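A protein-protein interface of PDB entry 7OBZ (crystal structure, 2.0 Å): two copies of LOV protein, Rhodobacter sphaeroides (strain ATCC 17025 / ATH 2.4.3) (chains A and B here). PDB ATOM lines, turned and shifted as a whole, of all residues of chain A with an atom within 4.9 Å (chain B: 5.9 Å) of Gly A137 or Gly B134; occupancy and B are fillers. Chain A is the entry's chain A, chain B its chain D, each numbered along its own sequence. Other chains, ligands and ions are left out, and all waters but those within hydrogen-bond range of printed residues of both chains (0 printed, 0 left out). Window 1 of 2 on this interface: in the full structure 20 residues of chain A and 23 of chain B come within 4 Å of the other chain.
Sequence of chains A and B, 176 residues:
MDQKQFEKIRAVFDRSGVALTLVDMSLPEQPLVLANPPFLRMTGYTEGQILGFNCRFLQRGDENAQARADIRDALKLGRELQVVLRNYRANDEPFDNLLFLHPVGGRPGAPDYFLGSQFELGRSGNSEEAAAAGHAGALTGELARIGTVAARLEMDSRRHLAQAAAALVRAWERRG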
ATOM      1  N   ALA A 133     -20.741 -31.551 -17.526  1.00  0.00           N
ATOM      2  CA  ALA A 133     -20.988 -30.123 -17.334  1.00  0.00           C
ATOM      3  C   ALA A 133     -22.393 -29.886 -16.800  1.00  0.00           C
ATOM      4  O   ALA A 133     -22.599 -29.067 -15.899  1.00  0.00           O
ATOM      5  CB  ALA A 133     -20.762 -29.364 -18.653  1.00  0.00           C
ATOM      6  N   GLY A 134     -23.368 -30.626 -17.321  1.00  0.00           N
ATOM      7  CA  GLY A 134     -24.705 -30.569 -16.757  1.00  0.00           C
ATOM      8  C   GLY A 134     -24.747 -30.955 -15.293  1.00  0.00           C
ATOM      9  O   GLY A 134     -25.475 -30.336 -14.501  1.00  0.00           O
ATOM     10  N   HIS A 135     -23.973 -31.987 -14.915  1.00  0.00           N
ATOM     11  CA  HIS A 135     -23.870 -32.368 -13.514  1.00  0.00           C
ATOM     12  C   HIS A 135     -23.300 -31.226 -12.686  1.00  0.00           C
ATOM     13  O   HIS A 135     -23.818 -30.905 -11.603  1.00  0.00           O
ATOM     14  CB  HIS A 135     -23.001 -33.632 -13.355  1.00  0.00           C
ATOM     15  CG  HIS A 135     -22.893 -34.097 -11.936  1.00  0.00           C
ATOM     16  ND1 HIS A 135     -23.649 -35.132 -11.426  1.00  0.00           N
ATOM     17  CD2 HIS A 135     -22.140 -33.641 -10.907  1.00  0.00           C
ATOM     18  CE1 HIS A 135     -23.362 -35.296 -10.147  1.00  0.00           C
ATOM     19  NE2 HIS A 135     -22.447 -34.405  -9.808  1.00  0.00           N
ATOM     20  N   ALA A 136     -22.227 -30.600 -13.193  1.00  0.00           N
ATOM     21  CA  ALA A 136     -21.597 -29.480 -12.495  1.00  0.00           C
ATOM     22  C   ALA A 136     -22.567 -28.319 -12.318  1.00  0.00           C
ATOM     23  O   ALA A 136     -22.542 -27.634 -11.293  1.00  0.00           O
ATOM     24  CB  ALA A 136     -20.357 -29.023 -13.261  1.00  0.00           C
ATOM     25  N   GLY A 137     -23.436 -28.105 -13.300  1.00  0.00           N
ATOM     26  CA  GLY A 137     -24.424 -27.050 -13.183  1.00  0.00           C
ATOM     27  C   GLY A 137     -25.415 -27.309 -12.065  1.00  0.00           C
ATOM     28  O   GLY A 137     -25.677 -26.428 -11.240  1.00  0.00           O
ATOM     29  N   ALA A 138     -25.970 -28.533 -12.016  1.00  0.00           N
ATOM     30  CA  ALA A 138     -26.879 -28.909 -10.934  1.00  0.00           C
ATOM     31  C   ALA A 138     -26.186 -28.821  -9.576  1.00  0.00           C
ATOM     32  O   ALA A 138     -26.761 -28.316  -8.595  1.00  0.00           O
ATOM     33  CB  ALA A 138     -27.418 -30.312 -11.188  1.00  0.00           C
ATOM     34  N   LEU A 139     -24.931 -29.269  -9.508  1.00  0.00           N
ATOM     35  CA  LEU A 139     -24.193 -29.243  -8.246  1.00  0.00           C
ATOM     36  C   LEU A 139     -24.037 -27.820  -7.706  1.00  0.00           C
ATOM     37  O   LEU A 139     -24.332 -27.563  -6.529  1.00  0.00           O
ATOM     38  CB  LEU A 139     -22.829 -29.894  -8.444  1.00  0.00           C
ATOM     39  CG  LEU A 139     -21.832 -29.874  -7.292  1.00  0.00           C
ATOM     40  CD1 LEU A 139     -22.386 -30.502  -5.987  1.00  0.00           C
ATOM     41  CD2 LEU A 139     -20.590 -30.623  -7.741  1.00  0.00           C
ATOM     42  N   THR A 140     -23.505 -26.895  -8.540  1.00  0.00           N
ATOM     43  CA  THR A 140     -23.440 -25.475  -8.175  1.00  0.00           C
ATOM     44  C   THR A 140     -24.780 -24.959  -7.649  1.00  0.00           C
ATOM     45  O   THR A 140     -24.829 -24.246  -6.643  1.00  0.00           O
ATOM     46  CB  THR A 140     -22.992 -24.623  -9.385  1.00  0.00           C
ATOM     47  OG1 THR A 140     -21.706 -25.054  -9.838  1.00  0.00           O
ATOM     48  CG2 THR A 140     -22.869 -23.177  -8.987  1.00  0.00           C
ATOM     49  N   GLY A 141     -25.878 -25.329  -8.296  1.00  0.00           N
ATOM     50  CA  GLY A 141     -27.189 -25.007  -7.741  1.00  0.00           C
ATOM     51  C   GLY A 141     -27.363 -25.488  -6.314  1.00  0.00           C
ATOM     52  O   GLY A 141     -27.838 -24.746  -5.442  1.00  0.00           O
ATOM     53  N   ARG A 158     -20.756 -21.775 -11.691  1.00  0.00           N
ATOM     54  CA  ARG A 158     -21.272 -22.790 -12.598  1.00  0.00           C
ATOM     55  C   ARG A 158     -20.466 -22.825 -13.888  1.00  0.00           C
ATOM     56  O   ARG A 158     -19.989 -23.885 -14.307  1.00  0.00           O
ATOM     57  CB  ARG A 158     -22.747 -22.490 -12.876  1.00  0.00           C
ATOM     58  CG  ARG A 158     -23.377 -23.289 -13.972  1.00  0.00           C
ATOM     59  CD  ARG A 158     -24.880 -23.089 -13.962  1.00  0.00           C
ATOM     60  NE  ARG A 158     -25.270 -21.735 -14.360  1.00  0.00           N
ATOM     61  CZ  ARG A 158     -25.917 -20.880 -13.576  1.00  0.00           C
ATOM     62  NH1 ARG A 158     -26.235 -21.195 -12.328  1.00  0.00           N
ATOM     63  NH2 ARG A 158     -26.271 -19.686 -14.059  1.00  0.00           N
ATOM     64  N   ALA A 162     -18.484 -26.195 -14.729  1.00  0.00           N
ATOM     65  CA  ALA A 162     -18.817 -26.943 -15.938  1.00  0.00           C
ATOM     66  C   ALA A 162     -17.626 -27.037 -16.881  1.00  0.00           C
ATOM     67  O   ALA A 162     -17.446 -28.059 -17.557  1.00  0.00           O
ATOM     68  CB  ALA A 162     -20.010 -26.317 -16.661  1.00  0.00           C
ATOM     69  N   GLU B 129     -19.911 -24.059 -24.737  1.00  0.00           N
ATOM     70  CA  GLU B 129     -20.575 -25.347 -24.811  1.00  0.00           C
ATOM     71  C   GLU B 129     -20.729 -25.947 -23.413  1.00  0.00           C
ATOM     72  O   GLU B 129     -21.818 -26.380 -23.025  1.00  0.00           O
ATOM     73  CB  GLU B 129     -19.770 -26.263 -25.732  1.00  0.00           C
ATOM     74  CG  GLU B 129     -20.496 -27.508 -26.206  1.00  0.00           C
ATOM     75  CD  GLU B 129     -19.619 -28.400 -27.086  1.00  0.00           C
ATOM     76  OE1 GLU B 129     -18.662 -27.884 -27.711  1.00  0.00           O
ATOM     77  OE2 GLU B 129     -19.890 -29.621 -27.153  1.00  0.00           O
ATOM     78  N   ALA B 130     -19.649 -25.953 -22.632  1.00  0.00           N
ATOM     79  CA  ALA B 130     -19.760 -26.389 -21.252  1.00  0.00           C
ATOM     80  C   ALA B 130     -20.706 -25.487 -20.474  1.00  0.00           C
ATOM     81  O   ALA B 130     -21.565 -25.979 -19.734  1.00  0.00           O
ATOM     82  CB  ALA B 130     -18.377 -26.430 -20.599  1.00  0.00           C
ATOM     83  N   ALA B 131     -20.588 -24.163 -20.648  1.00  0.00           N
ATOM     84  CA  ALA B 131     -21.397 -23.244 -19.845  1.00  0.00           C
ATOM     85  C   ALA B 131     -22.880 -23.382 -20.163  1.00  0.00           C
ATOM     86  O   ALA B 131     -23.723 -23.315 -19.261  1.00  0.00           O
ATOM     87  CB  ALA B 131     -20.947 -21.796 -20.051  1.00  0.00           C
ATOM     88  N   ALA B 132     -23.223 -23.577 -21.435  1.00  0.00           N
ATOM     89  CA  ALA B 132     -24.617 -23.831 -21.752  1.00  0.00           C
ATOM     90  C   ALA B 132     -25.093 -25.129 -21.099  1.00  0.00           C
ATOM     91  O   ALA B 132     -26.195 -25.181 -20.541  1.00  0.00           O
ATOM     92  CB  ALA B 132     -24.822 -23.874 -23.263  1.00  0.00           C
ATOM     93  N   ALA B 133     -24.274 -26.187 -21.176  1.00  0.00           N
ATOM     94  CA  ALA B 133     -24.582 -27.453 -20.513  1.00  0.00           C
ATOM     95  C   ALA B 133     -24.775 -27.258 -19.015  1.00  0.00           C
ATOM     96  O   ALA B 133     -25.780 -27.697 -18.445  1.00  0.00           O
ATOM     97  CB  ALA B 133     -23.468 -28.459 -20.782  1.00  0.00           C
ATOM     98  N   GLY B 134     -23.815 -26.597 -18.367  1.00  0.00           N
ATOM     99  CA  GLY B 134     -23.997 -26.158 -16.997  1.00  0.00           C
ATOM    100  C   GLY B 134     -25.340 -25.512 -16.743  1.00  0.00           C
ATOM    101  O   GLY B 134     -26.040 -25.863 -15.788  1.00  0.00           O
ATOM    102  N   HIS B 135     -25.712 -24.541 -17.588  1.00  0.00           N
ATOM    103  CA  HIS B 135     -26.998 -23.876 -17.431  1.00  0.00           C
ATOM    104  C   HIS B 135     -28.133 -24.883 -17.494  1.00  0.00           C
ATOM    105  O   HIS B 135     -29.070 -24.827 -16.693  1.00  0.00           O
ATOM    106  CB  HIS B 135     -27.192 -22.795 -18.512  1.00  0.00           C
ATOM    107  CG  HIS B 135     -28.464 -22.021 -18.353  1.00  0.00           C
ATOM    108  ND1 HIS B 135     -28.502 -20.756 -17.807  1.00  0.00           N
ATOM    109  CD2 HIS B 135     -29.753 -22.360 -18.606  1.00  0.00           C
ATOM    110  CE1 HIS B 135     -29.754 -20.331 -17.770  1.00  0.00           C
ATOM    111  NE2 HIS B 135     -30.533 -21.289 -18.243  1.00  0.00           N
ATOM    112  N   ALA B 136     -28.066 -25.801 -18.456  1.00  0.00           N
ATOM    113  CA  ALA B 136     -29.132 -26.772 -18.632  1.00  0.00           C
ATOM    114  C   ALA B 136     -29.239 -27.708 -17.427  1.00  0.00           C
ATOM    115  O   ALA B 136     -30.347 -28.077 -17.032  1.00  0.00           O
ATOM    116  CB  ALA B 136     -28.895 -27.556 -19.924  1.00  0.00           C
ATOM    117  N   GLY B 137     -28.113 -28.051 -16.796  1.00  0.00           N
ATOM    118  CA  GLY B 137     -28.177 -28.891 -15.610  1.00  0.00           C
ATOM    119  C   GLY B 137     -28.779 -28.179 -14.414  1.00  0.00           C
ATOM    120  O   GLY B 137     -29.576 -28.764 -13.671  1.00  0.00           O
ATOM    121  N   ALA B 138     -28.405 -26.911 -14.210  1.00  0.00           N
ATOM    122  CA  ALA B 138     -29.030 -26.105 -13.166  1.00  0.00           C
ATOM    123  C   ALA B 138     -30.522 -25.934 -13.433  1.00  0.00           C
ATOM    124  O   ALA B 138     -31.342 -26.066 -12.521  1.00  0.00           O
ATOM    125  CB  ALA B 138     -28.337 -24.746 -13.060  1.00  0.00           C
ATOM    126  N   LEU B 139     -30.894 -25.677 -14.685  1.00  0.00           N
ATOM    127  CA  LEU B 139     -32.309 -25.538 -15.019  1.00  0.00           C
ATOM    128  C   LEU B 139     -33.084 -26.818 -14.731  1.00  0.00           C
ATOM    129  O   LEU B 139     -34.221 -26.760 -14.236  1.00  0.00           O
ATOM    130  CB  LEU B 139     -32.474 -25.148 -16.484  1.00  0.00           C
ATOM    131  CG  LEU B 139     -33.905 -25.024 -17.028  1.00  0.00           C
ATOM    132  CD1 LEU B 139     -34.736 -24.036 -16.240  1.00  0.00           C
ATOM    133  CD2 LEU B 139     -33.822 -24.575 -18.482  1.00  0.00           C
ATOM    134  N   ALA B 162     -28.805 -31.022 -21.313  1.00  0.00           N
ATOM    135  CA  ALA B 162     -27.462 -30.493 -21.498  1.00  0.00           C
ATOM    136  C   ALA B 162     -26.942 -30.802 -22.899  1.00  0.00           C
ATOM    137  O   ALA B 162     -26.265 -29.977 -23.517  1.00  0.00           O
ATOM    138  CB  ALA B 162     -26.519 -31.052 -20.437  1.00  0.00           C
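Among the printed residues, pairs that only touch across the chains: Gly A134 with Gly B137 (3.3 Å), Gly A137 with Gly B134 (3.3 Å), Ala A133 with Gly B134 (3.4 Å), Ala A162 with Ala B130 (3.5 Å), Gly A134 with Ala B133 (3.5 Å), Arg A158 with Gly B134 (3.5 Å), Ala A133 with Ala B133 (3.6 Å), Gly A137 with Ala B138 (3.6 Å), Ala A138 with Gly B137 (3.6 Å), Ala A133 with Ala B130 (3.6 Å), Ala A138 with Ala B138 (3.7 Å), Arg A158 with Ala B138 (3.9 Å) and Arg A158 with His B135 (3.99 Å).
Of chain B, only Gly B134 and Ala B138 come within 4 Å of Gly A137.
Printed residues of chain A within 4 Å of Gly B134: Ala A133 (3.4 Å), Gly A137 (3.3 Å) and Arg A158 (3.5 Å).
Of the printed residues of chain A, Gly B137 touches Gly A134 and Ala A138.
Of the printed residues of chain A, His B135 touches Arg A158.
Of the printed residues of chain B, Ala A133 touches Ala B130, Ala B133 and Gly B134.
Of the printed residues of chain A, Ala B138 touches Gly A137, Ala A138 and Arg A158.
The nearest residue of chain B that does not touch Gly A137 is Gly B137 (4.2 Å).
The nearest printed residue of chain A that does not touch Gly B134 is Ala A162 (4.004 Å).
Of the 11 printed residues of chain A, 6 touch a printed residue of chain B.
Printed residues of chain A that touch a printed residue of chain B: Ala A133, Gly A134, Gly A137, Ala A138, Arg A158 and Ala A162.
Hydrophobic or aromatic side chains of chain A within 4 Å of the printed part of chain B: Ala A133, Ala A138 and Ala A162.
Hydrophobic or aromatic side chains of chain B within 4 Å of the printed part of chain A: Ala B130, Ala B133 and Ala B138.
Among the printed residues, no Asp or Glu carboxylate lies within 4 Å of a Lys or Arg side-chain nitrogen of the other chain.
Ala B133 touches its own counterpart, Ala A133.
Ala A133 touches Gly B134, and with the chains exchanged Gly A134 touches Ala B133.
Gly A134 touches Gly B137, and with the chains exchanged Gly A137 touches Gly B134.
Ala B138 touches its own counterpart, Ala A138.
8 positions are printed for both chains.
Of the 13 pairs that touch across the chains among the printed residues, 8 have their exchanged pair printed and touching as well.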
